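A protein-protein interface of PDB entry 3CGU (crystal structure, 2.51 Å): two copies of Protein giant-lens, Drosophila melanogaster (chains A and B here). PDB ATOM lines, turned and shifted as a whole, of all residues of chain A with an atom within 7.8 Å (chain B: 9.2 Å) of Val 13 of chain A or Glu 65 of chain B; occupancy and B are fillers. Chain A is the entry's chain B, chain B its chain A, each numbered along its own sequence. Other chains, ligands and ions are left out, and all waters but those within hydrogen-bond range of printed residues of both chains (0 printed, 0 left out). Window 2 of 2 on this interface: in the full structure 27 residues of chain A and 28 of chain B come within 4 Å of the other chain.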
ATOM      1  N   VAL A  13      -2.991  -2.943   5.967  1.00  0.00           N
ATOM      2  CA  VAL A  13      -2.929  -1.895   7.027  1.00  0.00           C
ATOM      3  C   VAL A  13      -1.534  -1.313   7.128  1.00  0.00           C
ATOM      4  O   VAL A  13      -0.547  -2.049   7.124  1.00  0.00           O
ATOM      5  CB  VAL A  13      -3.311  -2.452   8.396  1.00  0.00           C
ATOM      6  CG1 VAL A  13      -3.358  -1.323   9.422  1.00  0.00           C
ATOM      7  CG2 VAL A  13      -4.652  -3.166   8.309  1.00  0.00           C
ATOM      8  N   ARG A  14      -1.462   0.011   7.232  1.00  0.00           N
ATOM      9  CA  ARG A  14      -0.183   0.710   7.256  1.00  0.00           C
ATOM     10  C   ARG A  14       0.579   0.461   8.562  1.00  0.00           C
ATOM     11  O   ARG A  14       0.049   0.666   9.654  1.00  0.00           O
ATOM     12  CB  ARG A  14      -0.384   2.208   7.022  1.00  0.00           C
ATOM     13  CG  ARG A  14       0.839   2.916   6.457  1.00  0.00           C
ATOM     14  CD  ARG A  14       0.474   4.307   5.974  1.00  0.00           C
ATOM     15  NE  ARG A  14       0.520   5.288   7.058  1.00  0.00           N
ATOM     16  CZ  ARG A  14       1.469   6.215   7.180  1.00  0.00           C
ATOM     17  NH1 ARG A  14       2.439   6.293   6.278  1.00  0.00           N
ATOM     18  NH2 ARG A  14       1.446   7.071   8.197  1.00  0.00           N
ATOM     19  N   ILE A  15       1.830   0.026   8.436  1.00  0.00           N
ATOM     20  CA  ILE A  15       2.631  -0.353   9.592  1.00  0.00           C
ATOM     21  C   ILE A  15       3.886   0.495   9.754  1.00  0.00           C
ATOM     22  O   ILE A  15       4.774   0.468   8.914  1.00  0.00           O
ATOM     23  CB  ILE A  15       3.055  -1.820   9.496  1.00  0.00           C
ATOM     24  CG1 ILE A  15       1.821  -2.726   9.453  1.00  0.00           C
ATOM     25  CG2 ILE A  15       3.975  -2.171  10.635  1.00  0.00           C
ATOM     26  CD1 ILE A  15       2.136  -4.216   9.397  1.00  0.00           C
ATOM     27  N   LEU A  16       3.963   1.241  10.846  1.00  0.00           N
ATOM     28  CA  LEU A  16       5.136   2.055  11.126  1.00  0.00           C
ATOM     29  C   LEU A  16       5.835   1.545  12.379  1.00  0.00           C
ATOM     30  O   LEU A  16       5.224   0.856  13.190  1.00  0.00           O
ATOM     31  CB  LEU A  16       4.737   3.521  11.312  1.00  0.00           C
ATOM     32  CG  LEU A  16       4.681   4.409  10.067  1.00  0.00           C
ATOM     33  CD1 LEU A  16       6.069   4.532   9.447  1.00  0.00           C
ATOM     34  CD2 LEU A  16       3.701   3.861   9.040  1.00  0.00           C
ATOM     35  N   ILE A  38      -2.367   2.710  17.571  1.00  0.00           N
ATOM     36  CA  ILE A  38      -3.141   2.739  16.342  1.00  0.00           C
ATOM     37  C   ILE A  38      -3.965   4.017  16.248  1.00  0.00           C
ATOM     38  O   ILE A  38      -4.752   4.339  17.144  1.00  0.00           O
ATOM     39  CB  ILE A  38      -4.086   1.529  16.270  1.00  0.00           C
ATOM     40  CG1 ILE A  38      -3.290   0.222  16.327  1.00  0.00           C
ATOM     41  CG2 ILE A  38      -4.934   1.581  15.034  1.00  0.00           C
ATOM     42  CD1 ILE A  38      -4.180  -0.997  16.499  1.00  0.00           C
ATOM     43  N   ASP A  39      -3.780   4.750  15.157  1.00  0.00           N
ATOM     44  CA  ASP A  39      -4.578   5.928  14.890  1.00  0.00           C
ATOM     45  C   ASP A  39      -5.609   5.615  13.821  1.00  0.00           C
ATOM     46  O   ASP A  39      -5.289   5.054  12.778  1.00  0.00           O
ATOM     47  CB  ASP A  39      -3.696   7.093  14.433  1.00  0.00           C
ATOM     48  CG  ASP A  39      -4.513   8.315  14.047  1.00  0.00           C
ATOM     49  OD1 ASP A  39      -4.328   8.855  12.925  1.00  0.00           O
ATOM     50  OD2 ASP A  39      -5.374   8.709  14.866  1.00  0.00           O
ATOM     51  N   LEU A  40      -6.853   5.991  14.079  1.00  0.00           N
ATOM     52  CA  LEU A  40      -7.942   5.709  13.159  1.00  0.00           C
ATOM     53  C   LEU A  40      -8.592   6.994  12.646  1.00  0.00           C
ATOM     54  O   LEU A  40      -9.784   7.013  12.350  1.00  0.00           O
ATOM     55  CB  LEU A  40      -8.997   4.864  13.868  1.00  0.00           C
ATOM     56  CG  LEU A  40      -8.580   3.497  14.412  1.00  0.00           C
ATOM     57  CD1 LEU A  40      -9.667   2.935  15.321  1.00  0.00           C
ATOM     58  CD2 LEU A  40      -8.321   2.558  13.247  1.00  0.00           C
ATOM     59  N   THR A  43      -6.561   8.004   7.380  1.00  0.00           N
ATOM     60  CA  THR A  43      -6.116   6.683   6.960  1.00  0.00           C
ATOM     61  C   THR A  43      -5.504   5.952   8.149  1.00  0.00           C
ATOM     62  O   THR A  43      -4.509   6.402   8.697  1.00  0.00           O
ATOM     63  CB  THR A  43      -5.105   6.755   5.800  1.00  0.00           C
ATOM     64  OG1 THR A  43      -5.769   7.229   4.613  1.00  0.00           O
ATOM     65  CG2 THR A  43      -4.491   5.373   5.534  1.00  0.00           C
ATOM     66  N   PRO A  44      -6.109   4.822   8.546  1.00  0.00           N
ATOM     67  CA  PRO A  44      -5.684   4.083   9.717  1.00  0.00           C
ATOM     68  C   PRO A  44      -4.212   3.689   9.641  1.00  0.00           C
ATOM     69  O   PRO A  44      -3.771   3.124   8.642  1.00  0.00           O
ATOM     70  CB  PRO A  44      -6.559   2.822   9.668  1.00  0.00           C
ATOM     71  CG  PRO A  44      -7.753   3.224   8.914  1.00  0.00           C
ATOM     72  CD  PRO A  44      -7.246   4.171   7.872  1.00  0.00           C
ATOM     73  N   TRP A  45      -3.450   3.992  10.686  1.00  0.00           N
ATOM     74  CA  TRP A  45      -2.098   3.487  10.766  1.00  0.00           C
ATOM     75  C   TRP A  45      -1.772   2.900  12.131  1.00  0.00           C
ATOM     76  O   TRP A  45      -2.389   3.248  13.148  1.00  0.00           O
ATOM     77  CB  TRP A  45      -1.057   4.531  10.344  1.00  0.00           C
ATOM     78  CG  TRP A  45      -1.086   5.848  11.060  1.00  0.00           C
ATOM     79  CD1 TRP A  45      -1.672   7.006  10.620  1.00  0.00           C
ATOM     80  CD2 TRP A  45      -0.456   6.168  12.311  1.00  0.00           C
ATOM     81  NE1 TRP A  45      -1.465   8.021  11.530  1.00  0.00           N
ATOM     82  CE2 TRP A  45      -0.722   7.537  12.576  1.00  0.00           C
ATOM     83  CE3 TRP A  45       0.288   5.431  13.243  1.00  0.00           C
ATOM     84  CZ2 TRP A  45      -0.271   8.180  13.732  1.00  0.00           C
ATOM     85  CZ3 TRP A  45       0.742   6.076  14.391  1.00  0.00           C
ATOM     86  CH2 TRP A  45       0.457   7.439  14.624  1.00  0.00           C
ATOM     87  N   ILE A  46      -0.807   1.990  12.124  1.00  0.00           N
ATOM     88  CA  ILE A  46      -0.370   1.305  13.310  1.00  0.00           C
ATOM     89  C   ILE A  46       1.098   1.567  13.500  1.00  0.00           C
ATOM     90  O   ILE A  46       1.902   1.212  12.640  1.00  0.00           O
ATOM     91  CB  ILE A  46      -0.522  -0.213  13.143  1.00  0.00           C
ATOM     92  CG1 ILE A  46      -1.989  -0.582  12.904  1.00  0.00           C
ATOM     93  CG2 ILE A  46       0.051  -0.947  14.345  1.00  0.00           C
ATOM     94  CD1 ILE A  46      -2.206  -2.025  12.460  1.00  0.00           C
ATOM     95  N   SER A  60      -2.758  -6.885  17.095  1.00  0.00           N
ATOM     96  CA  SER A  60      -2.816  -6.009  15.912  1.00  0.00           C
ATOM     97  C   SER A  60      -4.219  -5.711  15.371  1.00  0.00           C
ATOM     98  O   SER A  60      -4.362  -4.956  14.412  1.00  0.00           O
ATOM     99  CB  SER A  60      -1.963  -6.593  14.783  1.00  0.00           C
ATOM    100  OG  SER A  60      -0.624  -6.783  15.206  1.00  0.00           O
ATOM    101  N   LEU A  62      -7.755  -4.055  14.766  1.00  0.00           N
ATOM    102  CA  LEU A  62      -8.160  -2.666  14.790  1.00  0.00           C
ATOM    103  C   LEU A  62      -9.312  -2.453  15.750  1.00  0.00           C
ATOM    104  O   LEU A  62      -9.716  -1.318  15.997  1.00  0.00           O
ATOM    105  CB  LEU A  62      -8.573  -2.208  13.395  1.00  0.00           C
ATOM    106  CG  LEU A  62      -7.469  -2.142  12.343  1.00  0.00           C
ATOM    107  CD1 LEU A  62      -8.091  -1.916  10.971  1.00  0.00           C
ATOM    108  CD2 LEU A  62      -6.463  -1.048  12.671  1.00  0.00           C
ATOM    109  N   PRO B  59     -19.504  -4.559   2.757  1.00  0.00           N
ATOM    110  CA  PRO B  59     -18.266  -4.765   3.512  1.00  0.00           C
ATOM    111  C   PRO B  59     -18.423  -4.348   4.982  1.00  0.00           C
ATOM    112  O   PRO B  59     -19.265  -3.505   5.303  1.00  0.00           O
ATOM    113  CB  PRO B  59     -17.264  -3.846   2.803  1.00  0.00           C
ATOM    114  CG  PRO B  59     -17.891  -3.538   1.470  1.00  0.00           C
ATOM    115  CD  PRO B  59     -19.356  -3.531   1.714  1.00  0.00           C
ATOM    116  N   SER B  61     -15.276  -4.672   7.215  1.00  0.00           N
ATOM    117  CA  SER B  61     -13.932  -4.422   7.720  1.00  0.00           C
ATOM    118  C   SER B  61     -13.857  -3.022   8.355  1.00  0.00           C
ATOM    119  O   SER B  61     -14.617  -2.117   7.982  1.00  0.00           O
ATOM    120  CB  SER B  61     -12.908  -4.553   6.587  1.00  0.00           C
ATOM    121  OG  SER B  61     -11.574  -4.428   7.069  1.00  0.00           O
ATOM    122  N   LEU B  62     -12.954  -2.850   9.317  1.00  0.00           N
ATOM    123  CA  LEU B  62     -12.821  -1.575  10.007  1.00  0.00           C
ATOM    124  C   LEU B  62     -11.732  -0.749   9.355  1.00  0.00           C
ATOM    125  O   LEU B  62     -11.529   0.409   9.706  1.00  0.00           O
ATOM    126  CB  LEU B  62     -12.480  -1.787  11.480  1.00  0.00           C
ATOM    127  CG  LEU B  62     -13.543  -2.399  12.390  1.00  0.00           C
ATOM    128  CD1 LEU B  62     -12.953  -2.596  13.786  1.00  0.00           C
ATOM    129  CD2 LEU B  62     -14.784  -1.497  12.457  1.00  0.00           C
ATOM    130  N   GLY B  63     -11.023  -1.357   8.411  1.00  0.00           N
ATOM    131  CA  GLY B  63      -9.942  -0.672   7.712  1.00  0.00           C
ATOM    132  C   GLY B  63     -10.400  -0.076   6.395  1.00  0.00           C
ATOM    133  O   GLY B  63     -11.597   0.049   6.146  1.00  0.00           O
ATOM    134  N   VAL B  64      -9.445   0.284   5.547  1.00  0.00           N
ATOM    135  CA  VAL B  64      -9.761   0.946   4.288  1.00  0.00           C
ATOM    136  C   VAL B  64      -9.167   0.204   3.091  1.00  0.00           C
ATOM    137  O   VAL B  64      -9.219   0.674   1.955  1.00  0.00           O
ATOM    138  CB  VAL B  64      -9.281   2.409   4.309  1.00  0.00           C
ATOM    139  CG1 VAL B  64      -9.972   3.157   5.436  1.00  0.00           C
ATOM    140  CG2 VAL B  64      -7.763   2.475   4.476  1.00  0.00           C
ATOM    141  N   GLU B  65      -8.627  -0.978   3.366  1.00  0.00           N
ATOM    142  CA  GLU B  65      -7.932  -1.784   2.375  1.00  0.00           C
ATOM    143  C   GLU B  65      -8.850  -2.451   1.349  1.00  0.00           C
ATOM    144  O   GLU B  65      -8.424  -2.736   0.231  1.00  0.00           O
ATOM    145  CB  GLU B  65      -7.105  -2.844   3.093  1.00  0.00           C
ATOM    146  CG  GLU B  65      -6.154  -2.250   4.113  1.00  0.00           C
ATOM    147  CD  GLU B  65      -5.116  -1.353   3.463  1.00  0.00           C
ATOM    148  OE1 GLU B  65      -4.882  -0.228   3.964  1.00  0.00           O
ATOM    149  OE2 GLU B  65      -4.536  -1.777   2.441  1.00  0.00           O
ATOM    150  N   ASP B  66     -10.102  -2.702   1.725  1.00  0.00           N
ATOM    151  CA  ASP B  66     -11.030  -3.425   0.853  1.00  0.00           C
ATOM    152  C   ASP B  66     -11.392  -2.702  -0.447  1.00  0.00           C
ATOM    153  O   ASP B  66     -11.994  -3.299  -1.327  1.00  0.00           O
ATOM    154  CB  ASP B  66     -12.307  -3.812   1.614  1.00  0.00           C
ATOM    155  CG  ASP B  66     -13.039  -2.598   2.204  1.00  0.00           C
ATOM    156  OD1 ASP B  66     -14.070  -2.805   2.902  1.00  0.00           O
ATOM    157  OD2 ASP B  66     -12.593  -1.439   1.965  1.00  0.00           O
ATOM    158  N   GLY B  67     -11.044  -1.421  -0.567  1.00  0.00           N
ATOM    159  CA  GLY B  67     -11.428  -0.633  -1.735  1.00  0.00           C
ATOM    160  C   GLY B  67     -12.906  -0.249  -1.777  1.00  0.00           C
ATOM    161  O   GLY B  67     -13.411   0.165  -2.822  1.00  0.00           O
ATOM    162  N   HIS B  68     -13.602  -0.376  -0.648  1.00  0.00           N
ATOM    163  CA  HIS B  68     -15.022  -0.045  -0.585  1.00  0.00           C
ATOM    164  C   HIS B  68     -15.332   1.025   0.449  1.00  0.00           C
ATOM    165  O   HIS B  68     -16.495   1.270   0.778  1.00  0.00           O
ATOM    166  CB  HIS B  68     -15.827  -1.294  -0.236  1.00  0.00           C
ATOM    167  CG  HIS B  68     -16.029  -2.208  -1.396  1.00  0.00           C
ATOM    168  ND1 HIS B  68     -17.255  -2.383  -1.995  1.00  0.00           N
ATOM    169  CD2 HIS B  68     -15.149  -2.961  -2.100  1.00  0.00           C
ATOM    170  CE1 HIS B  68     -17.130  -3.227  -3.006  1.00  0.00           C
ATOM    171  NE2 HIS B  68     -15.861  -3.590  -3.092  1.00  0.00           N
ATOM    172  N   THR B  69     -14.277   1.635   0.974  1.00  0.00           N
ATOM    173  CA  THR B  69     -14.399   2.519   2.108  1.00  0.00           C
ATOM    174  C   THR B  69     -13.974   3.945   1.789  1.00  0.00           C
ATOM    175  O   THR B  69     -12.963   4.181   1.142  1.00  0.00           O
ATOM    176  CB  THR B  69     -13.528   2.023   3.282  1.00  0.00           C
ATOM    177  OG1 THR B  69     -13.933   0.700   3.659  1.00  0.00           O
ATOM    178  CG2 THR B  69     -13.664   2.982   4.491  1.00  0.00           C
ATOM    179  N   ILE B  70     -14.748   4.901   2.263  1.00  0.00           N
ATOM    180  CA  ILE B  70     -14.293   6.290   2.285  1.00  0.00           C
ATOM    181  C   ILE B  70     -14.026   6.705   3.718  1.00  0.00           C
ATOM    182  O   ILE B  70     -14.934   6.705   4.541  1.00  0.00           O
ATOM    183  CB  ILE B  70     -15.334   7.227   1.700  1.00  0.00           C
ATOM    184  CG1 ILE B  70     -15.544   6.880   0.226  1.00  0.00           C
ATOM    185  CG2 ILE B  70     -14.879   8.661   1.853  1.00  0.00           C
ATOM    186  CD1 ILE B  70     -16.855   7.339  -0.316  1.00  0.00           C
ATOM    187  N   ALA B  71     -12.775   7.025   4.018  1.00  0.00           N
ATOM    188  CA  ALA B  71     -12.394   7.461   5.361  1.00  0.00           C
ATOM    189  C   ALA B  71     -12.630   8.961   5.488  1.00  0.00           C
ATOM    190  O   ALA B  71     -12.254   9.716   4.601  1.00  0.00           O
ATOM    191  CB  ALA B  71     -10.926   7.132   5.627  1.00  0.00           C
ATOM    192  N   HIS B  76     -16.026   6.003   8.847  1.00  0.00           N
ATOM    193  CA  HIS B  76     -15.820   5.284   7.591  1.00  0.00           C
ATOM    194  C   HIS B  76     -17.153   5.094   6.893  1.00  0.00           C
ATOM    195  O   HIS B  76     -18.145   4.749   7.519  1.00  0.00           O
ATOM    196  CB  HIS B  76     -15.217   3.906   7.843  1.00  0.00           C
ATOM    197  CG  HIS B  76     -13.786   3.944   8.275  1.00  0.00           C
ATOM    198  ND1 HIS B  76     -13.207   5.071   8.816  1.00  0.00           N
ATOM    199  CD2 HIS B  76     -12.822   2.984   8.274  1.00  0.00           C
ATOM    200  CE1 HIS B  76     -11.943   4.808   9.115  1.00  0.00           C
ATOM    201  NE2 HIS B  76     -11.685   3.547   8.799  1.00  0.00           N
ATOM    202  N   LYS B  78     -18.980   2.865   3.982  1.00  0.00           N
ATOM    203  CA  LYS B  78     -18.843   1.686   3.140  1.00  0.00           C
ATOM    204  C   LYS B  78     -19.723   1.821   1.924  1.00  0.00           C
ATOM    205  O   LYS B  78     -20.910   2.128   2.051  1.00  0.00           O
ATOM    206  CB  LYS B  78     -19.264   0.448   3.916  1.00  0.00           C
ATOM    207  CG  LYS B  78     -18.647   0.373   5.296  1.00  0.00           C
ATOM    208  CD  LYS B  78     -17.120   0.265   5.229  1.00  0.00           C
ATOM    209  CE  LYS B  78     -16.700  -1.144   4.894  1.00  0.00           C
ATOM    210  NZ  LYS B  78     -15.234  -1.369   5.119  1.00  0.00           N
ATOM    211  N   VAL B  83     -14.681   2.093  -4.525  1.00  0.00           N
ATOM    212  CA  VAL B  83     -14.612   3.554  -4.415  1.00  0.00           C
ATOM    213  C   VAL B  83     -13.874   4.254  -5.554  1.00  0.00           C
ATOM    214  O   VAL B  83     -14.085   5.443  -5.782  1.00  0.00           O
ATOM    215  CB  VAL B  83     -14.048   4.043  -3.042  1.00  0.00           C
ATOM    216  CG1 VAL B  83     -15.055   3.783  -1.938  1.00  0.00           C
ATOM    217  CG2 VAL B  83     -12.712   3.390  -2.732  1.00  0.00           C
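The side-chain hydroxyl (OG) of Ser 61 of chain B lies close to the backbone NH (N) of Gly 63 of chain B, at 3.4 Å. O of Gly 63 of chain B is in hydrogen-bond range of OG1 of Thr 69 of chain B (3.5 Å). O of Leu 62 of chain B lies close to NE2 of His 76 of chain B (3.3 Å).
Glu 65 of chain B touches Val 13 of chain A. CD of Pro 44 of chain A touches CG1 of Val 64 of chain B, at 3.8 Å. His 76 of chain B touches Pro 44 of chain A (NE2 to CG, 3.9 Å). Gly 63 of chain B touches Leu 62 of chain A.
Of chain B, only Glu 65 comes within 4 Å of Val 13 of chain A. Of chain A, only Val 13 (3.6 Å) comes within 4 Å of Glu 65 of chain B. Of the printed residues of chain B, Pro 44 of chain A touches Val 64 (3.8 Å) and His 76 (3.9 Å). Of the printed residues of chain A, His 76 of chain B touches Pro 44 (3.9 Å). Printed residues of chain A within 4 Å of Gly 63 of chain B: Leu 62 (3.9 Å). Ser 60 of chain A touches none of the printed residues of chain B. Ile 46 of chain A touches none of the printed residues of chain B. The nearest residue of chain B that does not touch Val 13 of chain A is Gly 63 of chain B (5.9 Å). The nearest residue of chain A that does not touch Glu 65 of chain B is Arg 14 of chain A (4.7 Å). The nearest printed residue of chain A that does not touch Gly 63 of chain B is Pro 44 of chain A (4.6 Å).
Of the 15 printed residues of chain B, 4 touch a printed residue of chain A. Printed residues of chain B that touch a printed residue of chain A: Gly 63, Val 64, Glu 65 and His 76. Hydrophobic or aromatic side chains of chain B that line the printed part of chain A: Val 64 and His 76. Of the 13 printed residues of chain A, 3 touch a printed residue of chain B. Hydrophobic or aromatic side chains of chain A within 4 Å of the printed part of chain B: Pro 44 and Leu 62. Along chain A the printed residues that touch a printed residue of chain B span positions 13 to 62. Among the printed residues, no Asp or Glu carboxylate lies within 4 Å of a Lys or Arg side-chain nitrogen of the other chain.
Position printed for both chains: 62. Of the 4 pairs that touch across the chains among the printed residues, none has its exchanged pair printed and touching as well.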
